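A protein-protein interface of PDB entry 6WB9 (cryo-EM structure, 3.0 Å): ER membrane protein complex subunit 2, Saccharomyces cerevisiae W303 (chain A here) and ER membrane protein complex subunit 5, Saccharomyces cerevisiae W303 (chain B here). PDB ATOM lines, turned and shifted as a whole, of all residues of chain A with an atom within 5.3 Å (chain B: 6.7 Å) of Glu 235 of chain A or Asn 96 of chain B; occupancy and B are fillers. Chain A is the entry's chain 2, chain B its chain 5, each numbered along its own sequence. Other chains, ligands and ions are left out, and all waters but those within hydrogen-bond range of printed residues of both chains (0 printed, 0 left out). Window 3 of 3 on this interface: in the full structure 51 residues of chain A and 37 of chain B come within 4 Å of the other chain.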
ATOM      1  N   LEU A 231      30.138   9.720  14.540  1.00  0.00           N
ATOM      2  CA  LEU A 231      29.405  10.780  15.216  1.00  0.00           C
ATOM      3  C   LEU A 231      30.231  12.049  15.341  1.00  0.00           C
ATOM      4  O   LEU A 231      29.668  13.148  15.358  1.00  0.00           O
ATOM      5  CB  LEU A 231      28.945  10.310  16.596  1.00  0.00           C
ATOM      6  CG  LEU A 231      27.746   9.363  16.600  1.00  0.00           C
ATOM      7  CD1 LEU A 231      27.658   8.643  17.923  1.00  0.00           C
ATOM      8  CD2 LEU A 231      26.465  10.112  16.312  1.00  0.00           C
ATOM      9  N   ARG A 232      31.555  11.926  15.438  1.00  0.00           N
ATOM     10  CA  ARG A 232      32.391  13.119  15.384  1.00  0.00           C
ATOM     11  C   ARG A 232      32.429  13.710  13.980  1.00  0.00           C
ATOM     12  O   ARG A 232      32.588  14.926  13.826  1.00  0.00           O
ATOM     13  CB  ARG A 232      33.801  12.796  15.870  1.00  0.00           C
ATOM     14  CG  ARG A 232      34.657  14.021  16.138  1.00  0.00           C
ATOM     15  CD  ARG A 232      34.014  14.933  17.161  1.00  0.00           C
ATOM     16  NE  ARG A 232      34.331  16.339  16.929  1.00  0.00           N
ATOM     17  CZ  ARG A 232      35.442  16.936  17.346  1.00  0.00           C
ATOM     18  NH1 ARG A 232      36.357  16.252  18.014  1.00  0.00           N
ATOM     19  NH2 ARG A 232      35.643  18.219  17.090  1.00  0.00           N
ATOM     20  N   SER A 233      32.268  12.875  12.948  1.00  0.00           N
ATOM     21  CA  SER A 233      32.237  13.387  11.581  1.00  0.00           C
ATOM     22  C   SER A 233      30.984  14.205  11.308  1.00  0.00           C
ATOM     23  O   SER A 233      31.005  15.095  10.452  1.00  0.00           O
ATOM     24  CB  SER A 233      32.328  12.241  10.579  1.00  0.00           C
ATOM     25  OG  SER A 233      31.183  11.416  10.648  1.00  0.00           O
ATOM     26  N   VAL A 234      29.887  13.930  12.016  1.00  0.00           N
ATOM     27  CA  VAL A 234      28.670  14.716  11.850  1.00  0.00           C
ATOM     28  C   VAL A 234      28.485  15.757  12.940  1.00  0.00           C
ATOM     29  O   VAL A 234      27.541  16.556  12.858  1.00  0.00           O
ATOM     30  CB  VAL A 234      27.416  13.824  11.768  1.00  0.00           C
ATOM     31  CG1 VAL A 234      27.443  13.026  10.495  1.00  0.00           C
ATOM     32  CG2 VAL A 234      27.327  12.920  12.974  1.00  0.00           C
ATOM     33  N   GLU A 235      29.344  15.778  13.953  1.00  0.00           N
ATOM     34  CA  GLU A 235      29.416  16.931  14.834  1.00  0.00           C
ATOM     35  C   GLU A 235      30.268  18.041  14.237  1.00  0.00           C
ATOM     36  O   GLU A 235      30.257  19.164  14.751  1.00  0.00           O
ATOM     37  CB  GLU A 235      29.971  16.522  16.197  1.00  0.00           C
ATOM     38  CG  GLU A 235      29.459  17.357  17.350  1.00  0.00           C
ATOM     39  CD  GLU A 235      30.386  17.323  18.540  1.00  0.00           C
ATOM     40  OE1 GLU A 235      31.376  16.564  18.500  1.00  0.00           O
ATOM     41  OE2 GLU A 235      30.128  18.056  19.516  1.00  0.00           O
ATOM     42  N   LEU A 236      31.005  17.746  13.169  1.00  0.00           N
ATOM     43  CA  LEU A 236      31.759  18.737  12.423  1.00  0.00           C
ATOM     44  C   LEU A 236      31.097  19.117  11.108  1.00  0.00           C
ATOM     45  O   LEU A 236      31.570  20.043  10.445  1.00  0.00           O
ATOM     46  CB  LEU A 236      33.174  18.223  12.138  1.00  0.00           C
ATOM     47  CG  LEU A 236      34.080  18.002  13.342  1.00  0.00           C
ATOM     48  CD1 LEU A 236      35.419  17.491  12.879  1.00  0.00           C
ATOM     49  CD2 LEU A 236      34.240  19.290  14.113  1.00  0.00           C
ATOM     50  N   SER A 237      30.029  18.425  10.715  1.00  0.00           N
ATOM     51  CA  SER A 237      29.335  18.718   9.464  1.00  0.00           C
ATOM     52  C   SER A 237      27.923  18.166   9.555  1.00  0.00           C
ATOM     53  O   SER A 237      27.750  16.952   9.665  1.00  0.00           O
ATOM     54  CB  SER A 237      30.071  18.106   8.280  1.00  0.00           C
ATOM     55  OG  SER A 237      29.476  18.501   7.062  1.00  0.00           O
ATOM     56  N   GLU A 238      26.924  19.048   9.492  1.00  0.00           N
ATOM     57  CA  GLU A 238      25.536  18.626   9.665  1.00  0.00           C
ATOM     58  C   GLU A 238      25.061  17.760   8.504  1.00  0.00           C
ATOM     59  O   GLU A 238      24.495  16.683   8.714  1.00  0.00           O
ATOM     60  CB  GLU A 238      24.631  19.847   9.815  1.00  0.00           C
ATOM     61  CG  GLU A 238      23.150  19.518   9.812  1.00  0.00           C
ATOM     62  CD  GLU A 238      22.280  20.725   9.538  1.00  0.00           C
ATOM     63  OE1 GLU A 238      22.822  21.766   9.113  1.00  0.00           O
ATOM     64  OE2 GLU A 238      21.052  20.632   9.742  1.00  0.00           O
ATOM     65  N   LEU A 239      25.288  18.210   7.272  1.00  0.00           N
ATOM     66  CA  LEU A 239      24.806  17.515   6.089  1.00  0.00           C
ATOM     67  C   LEU A 239      25.822  16.542   5.512  1.00  0.00           C
ATOM     68  O   LEU A 239      25.780  16.266   4.307  1.00  0.00           O
ATOM     69  CB  LEU A 239      24.393  18.521   5.015  1.00  0.00           C
ATOM     70  CG  LEU A 239      23.168  19.381   5.304  1.00  0.00           C
ATOM     71  CD1 LEU A 239      22.845  20.229   4.092  1.00  0.00           C
ATOM     72  CD2 LEU A 239      21.986  18.514   5.682  1.00  0.00           C
ATOM     73  N   ILE B  93      28.915  30.726  10.614  1.00  0.00           N
ATOM     74  CA  ILE B  93      30.207  30.547  11.255  1.00  0.00           C
ATOM     75  C   ILE B  93      30.344  29.178  11.909  1.00  0.00           C
ATOM     76  O   ILE B  93      31.460  28.665  12.017  1.00  0.00           O
ATOM     77  CB  ILE B  93      30.469  31.674  12.265  1.00  0.00           C
ATOM     78  CG1 ILE B  93      29.375  31.733  13.326  1.00  0.00           C
ATOM     79  CG2 ILE B  93      30.544  32.992  11.550  1.00  0.00           C
ATOM     80  CD1 ILE B  93      29.804  32.429  14.579  1.00  0.00           C
ATOM     81  N   ALA B  94      29.240  28.570  12.337  1.00  0.00           N
ATOM     82  CA  ALA B  94      29.301  27.278  13.006  1.00  0.00           C
ATOM     83  C   ALA B  94      29.663  26.190  12.007  1.00  0.00           C
ATOM     84  O   ALA B  94      29.035  26.076  10.952  1.00  0.00           O
ATOM     85  CB  ALA B  94      27.967  26.961  13.673  1.00  0.00           C
ATOM     86  N   LEU B  95      30.674  25.385  12.355  1.00  0.00           N
ATOM     87  CA  LEU B  95      31.236  24.395  11.441  1.00  0.00           C
ATOM     88  C   LEU B  95      30.248  23.291  11.078  1.00  0.00           C
ATOM     89  O   LEU B  95      30.415  22.654  10.033  1.00  0.00           O
ATOM     90  CB  LEU B  95      32.501  23.796  12.056  1.00  0.00           C
ATOM     91  CG  LEU B  95      33.463  23.019  11.159  1.00  0.00           C
ATOM     92  CD1 LEU B  95      33.993  23.890  10.038  1.00  0.00           C
ATOM     93  CD2 LEU B  95      34.595  22.464  11.988  1.00  0.00           C
ATOM     94  N   ASN B  96      29.230  23.056  11.911  1.00  0.00           N
ATOM     95  CA  ASN B  96      28.109  22.209  11.515  1.00  0.00           C
ATOM     96  C   ASN B  96      27.411  22.771  10.285  1.00  0.00           C
ATOM     97  O   ASN B  96      27.112  22.041   9.335  1.00  0.00           O
ATOM     98  CB  ASN B  96      27.108  22.088  12.665  1.00  0.00           C
ATOM     99  CG  ASN B  96      27.730  21.555  13.928  1.00  0.00           C
ATOM    100  OD1 ASN B  96      27.693  20.355  14.187  1.00  0.00           O
ATOM    101  ND2 ASN B  96      28.290  22.446  14.739  1.00  0.00           N
ATOM    102  N   LYS B  97      27.158  24.077  10.283  1.00  0.00           N
ATOM    103  CA  LYS B  97      26.438  24.731   9.205  1.00  0.00           C
ATOM    104  C   LYS B  97      27.350  25.443   8.216  1.00  0.00           C
ATOM    105  O   LYS B  97      26.874  25.856   7.154  1.00  0.00           O
ATOM    106  CB  LYS B  97      25.431  25.732   9.783  1.00  0.00           C
ATOM    107  CG  LYS B  97      24.012  25.197   9.936  1.00  0.00           C
ATOM    108  CD  LYS B  97      23.875  24.230  11.100  1.00  0.00           C
ATOM    109  CE  LYS B  97      24.127  24.917  12.426  1.00  0.00           C
ATOM    110  NZ  LYS B  97      23.905  23.996  13.575  1.00  0.00           N
ATOM    111  N   ALA B  98      28.637  25.600   8.533  1.00  0.00           N
ATOM    112  CA  ALA B  98      29.556  26.206   7.576  1.00  0.00           C
ATOM    113  C   ALA B  98      29.862  25.253   6.435  1.00  0.00           C
ATOM    114  O   ALA B  98      30.002  25.676   5.282  1.00  0.00           O
ATOM    115  CB  ALA B  98      30.849  26.623   8.269  1.00  0.00           C
ATOM    116  N   THR B  99      29.970  23.967   6.738  1.00  0.00           N
ATOM    117  CA  THR B  99      30.254  22.942   5.748  1.00  0.00           C
ATOM    118  C   THR B  99      29.003  22.442   5.045  1.00  0.00           C
ATOM    119  O   THR B  99      29.097  21.523   4.223  1.00  0.00           O
ATOM    120  CB  THR B  99      30.978  21.775   6.410  1.00  0.00           C
ATOM    121  OG1 THR B  99      30.181  21.290   7.491  1.00  0.00           O
ATOM    122  CG2 THR B  99      32.314  22.231   6.956  1.00  0.00           C
ATOM    123  N   ASN B 100      27.839  23.023   5.343  1.00  0.00           N
ATOM    124  CA  ASN B 100      26.638  22.711   4.579  1.00  0.00           C
ATOM    125  C   ASN B 100      26.756  23.195   3.144  1.00  0.00           C
ATOM    126  O   ASN B 100      26.195  22.573   2.242  1.00  0.00           O
ATOM    127  CB  ASN B 100      25.409  23.327   5.242  1.00  0.00           C
ATOM    128  CG  ASN B 100      24.928  22.524   6.425  1.00  0.00           C
ATOM    129  OD1 ASN B 100      25.595  21.592   6.867  1.00  0.00           O
ATOM    130  ND2 ASN B 100      23.764  22.883   6.949  1.00  0.00           N
ATOM    131  N   ASN B 103      28.826  20.478   1.504  1.00  0.00           N
ATOM    132  CA  ASN B 103      28.093  19.231   1.333  1.00  0.00           C
ATOM    133  C   ASN B 103      26.933  19.351   0.354  1.00  0.00           C
ATOM    134  O   ASN B 103      26.549  18.348  -0.259  1.00  0.00           O
ATOM    135  CB  ASN B 103      27.572  18.738   2.682  1.00  0.00           C
ATOM    136  CG  ASN B 103      28.685  18.405   3.645  1.00  0.00           C
ATOM    137  OD1 ASN B 103      29.676  17.782   3.275  1.00  0.00           O
ATOM    138  ND2 ASN B 103      28.533  18.830   4.889  1.00  0.00           N
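Asn 96 of chain B touches Ser 237 of chain A. Lys 97 of chain B touches Glu 238 of chain A. Asn 103 of chain B touches Leu 239 of chain A.
O of Glu 235 of chain A lies close to OD1 of Asn 96 of chain B (2.9 Å). O of Leu 236 of chain A lies within hydrogen-bond range of OG1 of Thr 99 of chain B (3.5 Å). The side-chain hydroxyl (OG) of Ser 237 of chain A lies within hydrogen-bond range of the side-chain hydroxyl (OG1) of Thr 99 of chain B. The backbone carbonyl oxygen (O) of Asn 96 of chain B lies within hydrogen-bond range of the backbone NH (N) of Glu 238 of chain A (3.0 Å). ND2 of Asn 100 of chain B is in hydrogen-bond range of OE1 of Glu 238 of chain A (2.6 Å). N of Leu 239 of chain A sits at hydrogen-bond distance from OD1 of Asn 100 of chain B. The backbone carbonyl oxygen (O) of Leu 236 of chain A lies close to the backbone carbonyl oxygen (O) of Leu 95 of chain B. The side-chain amide nitrogen of Asn 103 of chain B lies close to the side-chain hydroxyl of Ser 237 of chain A.
Hydrophobic or aromatic side chains of chain B within 4 Å of the printed part of chain A: Leu 95. Hydrophobic or aromatic side chains of chain A that line the printed part of chain B: Leu 236 and Leu 239.
Of the printed residues of chain B, Ser 237 of chain A touches Asn 96, Thr 99 and Asn 103. Of the printed residues of chain B, Glu 238 of chain A touches Asn 96 (3.0 Å), Lys 97 (3.3 Å) and Asn 100 (2.6 Å). Ala 94 of chain B touches none of the printed residues of chain A. Printed residues of chain A within 4 Å of Leu 95 of chain B: Leu 236. Of chain A, only Glu 235, Ser 237 and Glu 238 come within 4 Å of Asn 96 of chain B. Of the printed residues of chain A, Lys 97 of chain B touches Glu 238 (3.3 Å). Of the printed residues of chain A, Thr 99 of chain B touches Leu 236 (3.5 Å) and Ser 237 (2.9 Å). The nearest residue of chain B that does not touch Glu 235 of chain A is Leu 95 of chain B (5.5 Å). The nearest residue of chain A that does not touch Asn 96 of chain B is Val 234 of chain A (4.03 Å).
The side-chain carboxylate of Glu 235 of chain A lies within salt-bridge range of the guanidinium group of Arg 232 of chain A (3.4 Å). O of Leu 95 of chain B is in hydrogen-bond range of OG1 of Thr 99 of chain B, at 2.9 Å. The backbone carbonyl oxygen of Asn 96 of chain B sits close to the side-chain amide oxygen of Asn 100 of chain B (2.9 Å). O of Thr 99 of chain B lies within hydrogen-bond range of ND2 of Asn 103 of chain B.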
